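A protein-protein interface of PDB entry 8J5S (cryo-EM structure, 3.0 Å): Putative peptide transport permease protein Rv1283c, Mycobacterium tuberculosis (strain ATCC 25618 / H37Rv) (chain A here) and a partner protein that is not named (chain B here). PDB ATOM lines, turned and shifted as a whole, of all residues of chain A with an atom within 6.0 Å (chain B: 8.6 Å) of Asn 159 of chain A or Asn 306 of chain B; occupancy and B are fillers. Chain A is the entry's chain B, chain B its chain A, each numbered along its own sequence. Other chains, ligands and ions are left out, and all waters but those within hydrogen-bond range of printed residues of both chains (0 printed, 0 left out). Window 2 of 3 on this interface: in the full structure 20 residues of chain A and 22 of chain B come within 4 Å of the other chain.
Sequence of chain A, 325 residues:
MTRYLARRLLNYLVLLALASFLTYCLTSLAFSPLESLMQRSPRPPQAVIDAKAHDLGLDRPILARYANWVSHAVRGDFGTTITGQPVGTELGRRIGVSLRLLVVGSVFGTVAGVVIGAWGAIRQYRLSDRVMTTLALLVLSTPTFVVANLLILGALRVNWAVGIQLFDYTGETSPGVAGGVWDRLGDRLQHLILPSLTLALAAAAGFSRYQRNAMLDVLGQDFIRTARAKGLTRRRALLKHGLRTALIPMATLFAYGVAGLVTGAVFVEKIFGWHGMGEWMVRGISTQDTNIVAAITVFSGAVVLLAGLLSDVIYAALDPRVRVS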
ATOM      1  N   ALA A 155      -4.849 -14.151 -18.915  1.00  0.00           N
ATOM      2  CA  ALA A 155      -4.867 -13.190 -17.827  1.00  0.00           C
ATOM      3  C   ALA A 155      -5.535 -13.730 -16.579  1.00  0.00           C
ATOM      4  O   ALA A 155      -5.428 -13.106 -15.521  1.00  0.00           O
ATOM      5  CB  ALA A 155      -5.578 -11.919 -18.283  1.00  0.00           C
ATOM      6  N   LEU A 156      -6.241 -14.852 -16.679  1.00  0.00           N
ATOM      7  CA  LEU A 156      -6.672 -15.542 -15.468  1.00  0.00           C
ATOM      8  C   LEU A 156      -5.472 -16.015 -14.649  1.00  0.00           C
ATOM      9  O   LEU A 156      -5.439 -15.873 -13.414  1.00  0.00           O
ATOM     10  CB  LEU A 156      -7.563 -16.715 -15.860  1.00  0.00           C
ATOM     11  CG  LEU A 156      -8.194 -17.608 -14.806  1.00  0.00           C
ATOM     12  CD1 LEU A 156      -8.730 -16.767 -13.683  1.00  0.00           C
ATOM     13  CD2 LEU A 156      -9.304 -18.403 -15.451  1.00  0.00           C
ATOM     14  N   ARG A 157      -4.459 -16.564 -15.327  1.00  0.00           N
ATOM     15  CA  ARG A 157      -3.321 -17.155 -14.632  1.00  0.00           C
ATOM     16  C   ARG A 157      -2.467 -16.103 -13.946  1.00  0.00           C
ATOM     17  O   ARG A 157      -1.836 -16.395 -12.931  1.00  0.00           O
ATOM     18  CB  ARG A 157      -2.487 -17.970 -15.610  1.00  0.00           C
ATOM     19  CG  ARG A 157      -3.303 -18.875 -16.502  1.00  0.00           C
ATOM     20  CD  ARG A 157      -4.288 -19.682 -15.699  1.00  0.00           C
ATOM     21  NE  ARG A 157      -4.388 -21.060 -16.165  1.00  0.00           N
ATOM     22  CZ  ARG A 157      -5.233 -21.470 -17.101  1.00  0.00           C
ATOM     23  NH1 ARG A 157      -5.256 -22.744 -17.462  1.00  0.00           N
ATOM     24  NH2 ARG A 157      -6.060 -20.610 -17.671  1.00  0.00           N
ATOM     25  N   VAL A 158      -2.433 -14.883 -14.478  1.00  0.00           N
ATOM     26  CA  VAL A 158      -1.732 -13.792 -13.804  1.00  0.00           C
ATOM     27  C   VAL A 158      -2.356 -13.534 -12.440  1.00  0.00           C
ATOM     28  O   VAL A 158      -1.657 -13.383 -11.429  1.00  0.00           O
ATOM     29  CB  VAL A 158      -1.752 -12.525 -14.675  1.00  0.00           C
ATOM     30  CG1 VAL A 158      -1.371 -11.316 -13.856  1.00  0.00           C
ATOM     31  CG2 VAL A 158      -0.829 -12.678 -15.861  1.00  0.00           C
ATOM     32  N   ASN A 159      -3.689 -13.481 -12.398  1.00  0.00           N
ATOM     33  CA  ASN A 159      -4.397 -13.286 -11.139  1.00  0.00           C
ATOM     34  C   ASN A 159      -4.135 -14.437 -10.187  1.00  0.00           C
ATOM     35  O   ASN A 159      -4.028 -14.238  -8.974  1.00  0.00           O
ATOM     36  CB  ASN A 159      -5.893 -13.141 -11.399  1.00  0.00           C
ATOM     37  CG  ASN A 159      -6.324 -11.710 -11.475  1.00  0.00           C
ATOM     38  OD1 ASN A 159      -5.905 -10.890 -10.671  1.00  0.00           O
ATOM     39  ND2 ASN A 159      -7.162 -11.395 -12.446  1.00  0.00           N
ATOM     40  N   TRP A 160      -4.046 -15.654 -10.716  1.00  0.00           N
ATOM     41  CA  TRP A 160      -3.671 -16.775  -9.857  1.00  0.00           C
ATOM     42  C   TRP A 160      -2.270 -16.589  -9.279  1.00  0.00           C
ATOM     43  O   TRP A 160      -2.035 -16.860  -8.096  1.00  0.00           O
ATOM     44  CB  TRP A 160      -3.767 -18.091 -10.626  1.00  0.00           C
ATOM     45  CG  TRP A 160      -5.158 -18.471 -10.927  1.00  0.00           C
ATOM     46  CD1 TRP A 160      -6.277 -17.804 -10.557  1.00  0.00           C
ATOM     47  CD2 TRP A 160      -5.594 -19.608 -11.670  1.00  0.00           C
ATOM     48  NE1 TRP A 160      -7.390 -18.452 -11.020  1.00  0.00           N
ATOM     49  CE2 TRP A 160      -6.996 -19.567 -11.710  1.00  0.00           C
ATOM     50  CE3 TRP A 160      -4.935 -20.656 -12.310  1.00  0.00           C
ATOM     51  CZ2 TRP A 160      -7.755 -20.533 -12.362  1.00  0.00           C
ATOM     52  CZ3 TRP A 160      -5.693 -21.616 -12.959  1.00  0.00           C
ATOM     53  CH2 TRP A 160      -7.087 -21.547 -12.976  1.00  0.00           C
ATOM     54  N   ALA A 161      -1.328 -16.136 -10.104  1.00  0.00           N
ATOM     55  CA  ALA A 161       0.054 -15.996  -9.660  1.00  0.00           C
ATOM     56  C   ALA A 161       0.192 -14.935  -8.581  1.00  0.00           C
ATOM     57  O   ALA A 161       0.898 -15.145  -7.590  1.00  0.00           O
ATOM     58  CB  ALA A 161       0.956 -15.662 -10.845  1.00  0.00           C
ATOM     59  N   VAL A 162      -0.465 -13.793  -8.749  1.00  0.00           N
ATOM     60  CA  VAL A 162      -0.308 -12.690  -7.799  1.00  0.00           C
ATOM     61  C   VAL A 162      -1.317 -12.781  -6.660  1.00  0.00           C
ATOM     62  O   VAL A 162      -0.958 -12.636  -5.489  1.00  0.00           O
ATOM     63  CB  VAL A 162      -0.406 -11.340  -8.534  1.00  0.00           C
ATOM     64  CG1 VAL A 162      -0.126 -10.210  -7.574  1.00  0.00           C
ATOM     65  CG2 VAL A 162       0.568 -11.305  -9.690  1.00  0.00           C
ATOM     66  N   GLY A 163      -2.593 -13.009  -6.974  1.00  0.00           N
ATOM     67  CA  GLY A 163      -3.607 -13.251  -5.971  1.00  0.00           C
ATOM     68  C   GLY A 163      -4.340 -12.029  -5.460  1.00  0.00           C
ATOM     69  O   GLY A 163      -5.289 -12.183  -4.682  1.00  0.00           O
ATOM     70  N   ILE A 164      -3.938 -10.820  -5.866  1.00  0.00           N
ATOM     71  CA  ILE A 164      -4.590  -9.602  -5.395  1.00  0.00           C
ATOM     72  C   ILE A 164      -5.779  -9.214  -6.269  1.00  0.00           C
ATOM     73  O   ILE A 164      -6.410  -8.177  -6.024  1.00  0.00           O
ATOM     74  CB  ILE A 164      -3.541  -8.468  -5.298  1.00  0.00           C
ATOM     75  CG1 ILE A 164      -4.094  -7.203  -4.627  1.00  0.00           C
ATOM     76  CG2 ILE A 164      -2.987  -8.132  -6.664  1.00  0.00           C
ATOM     77  CD1 ILE A 164      -4.708  -7.429  -3.265  1.00  0.00           C
ATOM     78  N   GLN A 165      -6.132 -10.038  -7.258  1.00  0.00           N
ATOM     79  CA  GLN A 165      -7.225  -9.741  -8.186  1.00  0.00           C
ATOM     80  C   GLN A 165      -6.972  -8.416  -8.904  1.00  0.00           C
ATOM     81  O   GLN A 165      -7.732  -7.456  -8.783  1.00  0.00           O
ATOM     82  CB  GLN A 165      -8.579  -9.733  -7.468  1.00  0.00           C
ATOM     83  CG  GLN A 165      -9.135 -11.111  -7.159  1.00  0.00           C
ATOM     84  CD  GLN A 165      -9.923 -11.684  -8.310  1.00  0.00           C
ATOM     85  OE1 GLN A 165     -10.807 -11.031  -8.861  1.00  0.00           O
ATOM     86  NE2 GLN A 165      -9.602 -12.914  -8.687  1.00  0.00           N
ATOM     87  N   LEU A 166      -5.869  -8.382  -9.652  1.00  0.00           N
ATOM     88  CA  LEU A 166      -5.470  -7.154 -10.334  1.00  0.00           C
ATOM     89  C   LEU A 166      -6.512  -6.724 -11.352  1.00  0.00           C
ATOM     90  O   LEU A 166      -6.833  -5.536 -11.458  1.00  0.00           O
ATOM     91  CB  LEU A 166      -4.120  -7.339 -11.024  1.00  0.00           C
ATOM     92  CG  LEU A 166      -2.961  -7.949 -10.248  1.00  0.00           C
ATOM     93  CD1 LEU A 166      -2.895  -9.453 -10.459  1.00  0.00           C
ATOM     94  CD2 LEU A 166      -1.667  -7.293 -10.681  1.00  0.00           C
ATOM     95  N   PHE A 167      -7.042  -7.671 -12.119  1.00  0.00           N
ATOM     96  CA  PHE A 167      -8.045  -7.353 -13.121  1.00  0.00           C
ATOM     97  C   PHE A 167      -8.984  -8.534 -13.283  1.00  0.00           C
ATOM     98  O   PHE A 167      -8.583  -9.687 -13.128  1.00  0.00           O
ATOM     99  CB  PHE A 167      -7.407  -6.985 -14.464  1.00  0.00           C
ATOM    100  CG  PHE A 167      -6.280  -7.882 -14.868  1.00  0.00           C
ATOM    101  CD1 PHE A 167      -6.521  -9.185 -15.243  1.00  0.00           C
ATOM    102  CD2 PHE A 167      -4.979  -7.420 -14.890  1.00  0.00           C
ATOM    103  CE1 PHE A 167      -5.492 -10.010 -15.607  1.00  0.00           C
ATOM    104  CE2 PHE A 167      -3.945  -8.247 -15.264  1.00  0.00           C
ATOM    105  CZ  PHE A 167      -4.205  -9.541 -15.625  1.00  0.00           C
ATOM    106  N   ASP A 168     -10.241  -8.234 -13.582  1.00  0.00           N
ATOM    107  CA  ASP A 168     -11.211  -9.260 -13.911  1.00  0.00           C
ATOM    108  C   ASP A 168     -11.907  -8.885 -15.209  1.00  0.00           C
ATOM    109  O   ASP A 168     -11.706  -7.803 -15.757  1.00  0.00           O
ATOM    110  CB  ASP A 168     -12.200  -9.496 -12.760  1.00  0.00           C
ATOM    111  CG  ASP A 168     -13.345  -8.513 -12.733  1.00  0.00           C
ATOM    112  OD1 ASP A 168     -13.311  -7.487 -13.438  1.00  0.00           O
ATOM    113  OD2 ASP A 168     -14.300  -8.775 -11.975  1.00  0.00           O
ATOM    114  N   TYR A 169     -12.746  -9.796 -15.697  1.00  0.00           N
ATOM    115  CA  TYR A 169     -13.285  -9.693 -17.044  1.00  0.00           C
ATOM    116  C   TYR A 169     -14.784  -9.939 -17.084  1.00  0.00           C
ATOM    117  O   TYR A 169     -15.316 -10.290 -18.137  1.00  0.00           O
ATOM    118  CB  TYR A 169     -12.569 -10.675 -17.967  1.00  0.00           C
ATOM    119  CG  TYR A 169     -12.375 -12.030 -17.344  1.00  0.00           C
ATOM    120  CD1 TYR A 169     -11.246 -12.324 -16.609  1.00  0.00           C
ATOM    121  CD2 TYR A 169     -13.334 -13.014 -17.479  1.00  0.00           C
ATOM    122  CE1 TYR A 169     -11.075 -13.554 -16.039  1.00  0.00           C
ATOM    123  CE2 TYR A 169     -13.172 -14.246 -16.910  1.00  0.00           C
ATOM    124  CZ  TYR A 169     -12.043 -14.513 -16.192  1.00  0.00           C
ATOM    125  OH  TYR A 169     -11.883 -15.753 -15.623  1.00  0.00           O
ATOM    126  N   THR A 170     -15.474  -9.774 -15.968  1.00  0.00           N
ATOM    127  CA  THR A 170     -16.903 -10.039 -15.887  1.00  0.00           C
ATOM    128  C   THR A 170     -17.625  -8.722 -15.657  1.00  0.00           C
ATOM    129  O   THR A 170     -17.514  -8.125 -14.584  1.00  0.00           O
ATOM    130  CB  THR A 170     -17.212 -11.035 -14.774  1.00  0.00           C
ATOM    131  OG1 THR A 170     -16.700 -12.322 -15.132  1.00  0.00           O
ATOM    132  CG2 THR A 170     -18.704 -11.140 -14.554  1.00  0.00           C
ATOM    133  N   ARG B  92     -22.652 -14.547  -3.761  1.00  0.00           N
ATOM    134  CA  ARG B  92     -22.725 -14.177  -5.168  1.00  0.00           C
ATOM    135  C   ARG B  92     -23.014 -15.422  -5.992  1.00  0.00           C
ATOM    136  O   ARG B  92     -22.189 -16.333  -6.061  1.00  0.00           O
ATOM    137  CB  ARG B  92     -21.429 -13.520  -5.625  1.00  0.00           C
ATOM    138  CG  ARG B  92     -20.909 -12.476  -4.686  1.00  0.00           C
ATOM    139  CD  ARG B  92     -19.452 -12.198  -4.922  1.00  0.00           C
ATOM    140  NE  ARG B  92     -18.610 -13.212  -4.314  1.00  0.00           N
ATOM    141  CZ  ARG B  92     -17.423 -13.562  -4.781  1.00  0.00           C
ATOM    142  NH1 ARG B  92     -16.715 -14.493  -4.168  1.00  0.00           N
ATOM    143  NH2 ARG B  92     -16.941 -12.974  -5.857  1.00  0.00           N
ATOM    144  N   ARG B 300     -19.939 -18.197 -17.194  1.00  0.00           N
ATOM    145  CA  ARG B 300     -20.441 -18.502 -15.861  1.00  0.00           C
ATOM    146  C   ARG B 300     -19.431 -19.272 -15.033  1.00  0.00           C
ATOM    147  O   ARG B 300     -19.351 -19.074 -13.824  1.00  0.00           O
ATOM    148  CB  ARG B 300     -21.739 -19.299 -15.964  1.00  0.00           C
ATOM    149  CG  ARG B 300     -22.828 -18.847 -15.026  1.00  0.00           C
ATOM    150  CD  ARG B 300     -24.062 -19.712 -15.185  1.00  0.00           C
ATOM    151  NE  ARG B 300     -23.784 -21.112 -14.881  1.00  0.00           N
ATOM    152  CZ  ARG B 300     -23.745 -22.080 -15.788  1.00  0.00           C
ATOM    153  NH1 ARG B 300     -23.966 -21.800 -17.059  1.00  0.00           N
ATOM    154  NH2 ARG B 300     -23.482 -23.324 -15.421  1.00  0.00           N
ATOM    155  N   LEU B 301     -18.674 -20.154 -15.653  1.00  0.00           N
ATOM    156  CA  LEU B 301     -17.596 -20.884 -15.007  1.00  0.00           C
ATOM    157  C   LEU B 301     -16.341 -20.022 -14.921  1.00  0.00           C
ATOM    158  O   LEU B 301     -15.644 -20.090 -13.906  1.00  0.00           O
ATOM    159  CB  LEU B 301     -17.310 -22.203 -15.729  1.00  0.00           C
ATOM    160  CG  LEU B 301     -18.222 -23.374 -15.352  1.00  0.00           C
ATOM    161  CD1 LEU B 301     -18.049 -23.764 -13.902  1.00  0.00           C
ATOM    162  CD2 LEU B 301     -19.676 -23.044 -15.623  1.00  0.00           C
ATOM    163  N   PRO B 302     -15.992 -19.225 -15.938  1.00  0.00           N
ATOM    164  CA  PRO B 302     -14.933 -18.229 -15.726  1.00  0.00           C
ATOM    165  C   PRO B 302     -15.246 -17.262 -14.601  1.00  0.00           C
ATOM    166  O   PRO B 302     -14.335 -16.832 -13.881  1.00  0.00           O
ATOM    167  CB  PRO B 302     -14.860 -17.510 -17.076  1.00  0.00           C
ATOM    168  CG  PRO B 302     -15.319 -18.493 -18.043  1.00  0.00           C
ATOM    169  CD  PRO B 302     -16.367 -19.305 -17.360  1.00  0.00           C
ATOM    170  N   ALA B 303     -16.519 -16.911 -14.429  1.00  0.00           N
ATOM    171  CA  ALA B 303     -16.917 -16.070 -13.313  1.00  0.00           C
ATOM    172  C   ALA B 303     -16.605 -16.741 -11.986  1.00  0.00           C
ATOM    173  O   ALA B 303     -16.219 -16.076 -11.023  1.00  0.00           O
ATOM    174  CB  ALA B 303     -18.403 -15.748 -13.419  1.00  0.00           C
ATOM    175  N   LEU B 304     -16.780 -18.057 -11.911  1.00  0.00           N
ATOM    176  CA  LEU B 304     -16.410 -18.788 -10.705  1.00  0.00           C
ATOM    177  C   LEU B 304     -14.899 -18.864 -10.548  1.00  0.00           C
ATOM    178  O   LEU B 304     -14.380 -18.767  -9.432  1.00  0.00           O
ATOM    179  CB  LEU B 304     -17.012 -20.190 -10.744  1.00  0.00           C
ATOM    180  CG  LEU B 304     -16.965 -21.016  -9.465  1.00  0.00           C
ATOM    181  CD1 LEU B 304     -18.110 -20.658  -8.557  1.00  0.00           C
ATOM    182  CD2 LEU B 304     -17.003 -22.488  -9.801  1.00  0.00           C
ATOM    183  N   GLN B 305     -14.178 -19.044 -11.656  1.00  0.00           N
ATOM    184  CA  GLN B 305     -12.726 -19.160 -11.590  1.00  0.00           C
ATOM    185  C   GLN B 305     -12.092 -17.884 -11.064  1.00  0.00           C
ATOM    186  O   GLN B 305     -11.174 -17.936 -10.240  1.00  0.00           O
ATOM    187  CB  GLN B 305     -12.161 -19.497 -12.965  1.00  0.00           C
ATOM    188  CG  GLN B 305     -12.715 -20.755 -13.581  1.00  0.00           C
ATOM    189  CD  GLN B 305     -11.698 -21.490 -14.420  1.00  0.00           C
ATOM    190  OE1 GLN B 305     -10.852 -22.205 -13.902  1.00  0.00           O
ATOM    191  NE2 GLN B 305     -11.774 -21.313 -15.728  1.00  0.00           N
ATOM    192  N   ASN B 306     -12.562 -16.729 -11.526  1.00  0.00           N
ATOM    193  CA  ASN B 306     -11.978 -15.453 -11.137  1.00  0.00           C
ATOM    194  C   ASN B 306     -12.648 -14.838  -9.921  1.00  0.00           C
ATOM    195  O   ASN B 306     -12.494 -13.637  -9.691  1.00  0.00           O
ATOM    196  CB  ASN B 306     -12.021 -14.467 -12.302  1.00  0.00           C
ATOM    197  CG  ASN B 306     -10.831 -13.540 -12.315  1.00  0.00           C
ATOM    198  OD1 ASN B 306      -9.824 -13.797 -11.663  1.00  0.00           O
ATOM    199  ND2 ASN B 306     -10.937 -12.454 -13.058  1.00  0.00           N
ATOM    200  N   ASN B 307     -13.388 -15.627  -9.146  1.00  0.00           N
ATOM    201  CA  ASN B 307     -13.988 -15.176  -7.894  1.00  0.00           C
ATOM    202  C   ASN B 307     -14.915 -13.985  -8.126  1.00  0.00           C
ATOM    203  O   ASN B 307     -14.687 -12.879  -7.641  1.00  0.00           O
ATOM    204  CB  ASN B 307     -12.907 -14.839  -6.863  1.00  0.00           C
ATOM    205  CG  ASN B 307     -13.456 -14.690  -5.460  1.00  0.00           C
ATOM    206  OD1 ASN B 307     -14.495 -14.077  -5.245  1.00  0.00           O
ATOM    207  ND2 ASN B 307     -12.750 -15.253  -4.492  1.00  0.00           N
ATOM    208  N   THR B 308     -15.967 -14.224  -8.895  1.00  0.00           N
ATOM    209  CA  THR B 308     -17.071 -13.282  -8.982  1.00  0.00           C
ATOM    210  C   THR B 308     -18.394 -13.869  -8.524  1.00  0.00           C
ATOM    211  O   THR B 308     -19.263 -13.116  -8.086  1.00  0.00           O
ATOM    212  CB  THR B 308     -17.231 -12.747 -10.408  1.00  0.00           C
ATOM    213  OG1 THR B 308     -17.745 -13.783 -11.240  1.00  0.00           O
ATOM    214  CG2 THR B 308     -15.904 -12.272 -10.959  1.00  0.00           C
ATOM    215  N   ILE B 309     -18.571 -15.186  -8.610  1.00  0.00           N
ATOM    216  CA  ILE B 309     -19.725 -15.857  -8.023  1.00  0.00           C
ATOM    217  C   ILE B 309     -19.226 -16.928  -7.069  1.00  0.00           C
ATOM    218  O   ILE B 309     -18.019 -17.085  -6.874  1.00  0.00           O
ATOM    219  CB  ILE B 309     -20.652 -16.458  -9.091  1.00  0.00           C
ATOM    220  CG1 ILE B 309     -19.850 -17.247 -10.109  1.00  0.00           C
ATOM    221  CG2 ILE B 309     -21.442 -15.377  -9.783  1.00  0.00           C
ATOM    222  CD1 ILE B 309     -20.685 -17.764 -11.223  1.00  0.00           C
ATOM    223  N   THR B 326      -9.381 -26.310 -10.334  1.00  0.00           N
ATOM    224  CA  THR B 326      -9.059 -25.095  -9.610  1.00  0.00           C
ATOM    225  C   THR B 326      -9.124 -25.349  -8.114  1.00  0.00           C
ATOM    226  O   THR B 326      -9.602 -26.384  -7.649  1.00  0.00           O
ATOM    227  CB  THR B 326     -10.009 -23.968  -9.995  1.00  0.00           C
ATOM    228  OG1 THR B 326     -11.218 -24.111  -9.259  1.00  0.00           O
ATOM    229  CG2 THR B 326     -10.321 -24.042 -11.457  1.00  0.00           C
ATOM    230  N   ILE B 329     -12.610 -24.500  -4.654  1.00  0.00           N
ATOM    231  CA  ILE B 329     -13.945 -24.851  -5.122  1.00  0.00           C
ATOM    232  C   ILE B 329     -14.125 -26.353  -4.991  1.00  0.00           C
ATOM    233  O   ILE B 329     -13.289 -27.124  -5.471  1.00  0.00           O
ATOM    234  CB  ILE B 329     -14.169 -24.394  -6.574  1.00  0.00           C
ATOM    235  CG1 ILE B 329     -13.824 -22.914  -6.709  1.00  0.00           C
ATOM    236  CG2 ILE B 329     -15.594 -24.625  -6.983  1.00  0.00           C
ATOM    237  CD1 ILE B 329     -13.651 -22.458  -8.114  1.00  0.00           C
ATOM    238  N   ARG B 567     -18.006 -23.064  -3.715  1.00  0.00           N
ATOM    239  CA  ARG B 567     -16.756 -22.739  -3.045  1.00  0.00           C
ATOM    240  C   ARG B 567     -16.628 -23.556  -1.768  1.00  0.00           C
ATOM    241  O   ARG B 567     -17.589 -23.714  -1.015  1.00  0.00           O
ATOM    242  CB  ARG B 567     -16.695 -21.249  -2.731  1.00  0.00           C
ATOM    243  CG  ARG B 567     -15.361 -20.598  -3.041  1.00  0.00           C
ATOM    244  CD  ARG B 567     -15.484 -19.092  -3.155  1.00  0.00           C
ATOM    245  NE  ARG B 567     -15.789 -18.666  -4.514  1.00  0.00           N
ATOM    246  CZ  ARG B 567     -14.893 -18.571  -5.487  1.00  0.00           C
ATOM    247  NH1 ARG B 567     -13.627 -18.874  -5.260  1.00  0.00           N
ATOM    248  NH2 ARG B 567     -15.260 -18.173  -6.693  1.00  0.00           N
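Among the printed residues, merely in contact across the chains: Tyr 169 of chain A with Asn 306 of chain B (3.2 Å), Asp 168 of chain A with Asn 306 of chain B (3.2 Å), Phe 167 of chain A with Asn 306 of chain B (3.6 Å), Asn 159 of chain A with Asn 306 of chain B (3.7 Å), Leu 156 of chain A with Asn 306 of chain B (3.8 Å), Leu 156 of chain A with Gln 305 of chain B (3.8 Å), Trp 160 of chain A with Gln 305 of chain B (3.8 Å) and Asp 168 of chain A with Thr 308 of chain B (3.98 Å).
Of chain B, only Asn 306 comes within 4 Å of Asn 159 of chain A. Printed residues of chain B within 4 Å of Gln 165 of chain A: Asn 306. Of the printed residues of chain A, Pro 302 of chain B touches Tyr 169. Asn 306 of chain B touches just these residues of chain A: Leu 156, Asn 159, Gln 165, Phe 167, Asp 168 and Tyr 169. Of the printed residues of chain A, Thr 308 of chain B touches Asp 168. The nearest residue of chain A that does not touch Asn 306 of chain B is Trp 160 of chain A (5.3 Å).
The backbone carbonyl oxygen (O) of Pro 302 of chain B sits at hydrogen-bond distance from the side-chain hydroxyl (OH) of Tyr 169 of chain A. The side-chain amide oxygen (OD1) of Asn 306 of chain B lies within hydrogen-bond range of the side-chain amide nitrogen (NE2) of Gln 165 of chain A (3.1 Å).
The backbone carbonyl oxygen (O) of Ala 303 of chain B is in hydrogen-bond range of the side-chain hydroxyl (OG1) of Thr 308 of chain B (2.8 Å). The backbone NH of Leu 166 of chain A sits at hydrogen-bond distance from the side-chain amide oxygen of Asn 159 of chain A (2.7 Å). The guanidinium group (NH2) of Arg 92 of chain B lies close to the backbone carbonyl oxygen (O) of Thr 308 of chain B (3.2 Å).
Printed residues of chain A that touch a printed residue of chain B: Leu 156, Asn 159, Trp 160, Gln 165, Phe 167, Asp 168 and Tyr 169. Hydrophobic or aromatic side chains of chain A within 4 Å of the printed part of chain B: Leu 156, Trp 160 and Tyr 169. Among the printed residues, 10 pairs touch across the chains. Among the printed residues, no Asp or Glu carboxylate lies within 4 Å of a Lys or Arg side-chain nitrogen of the other chain.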
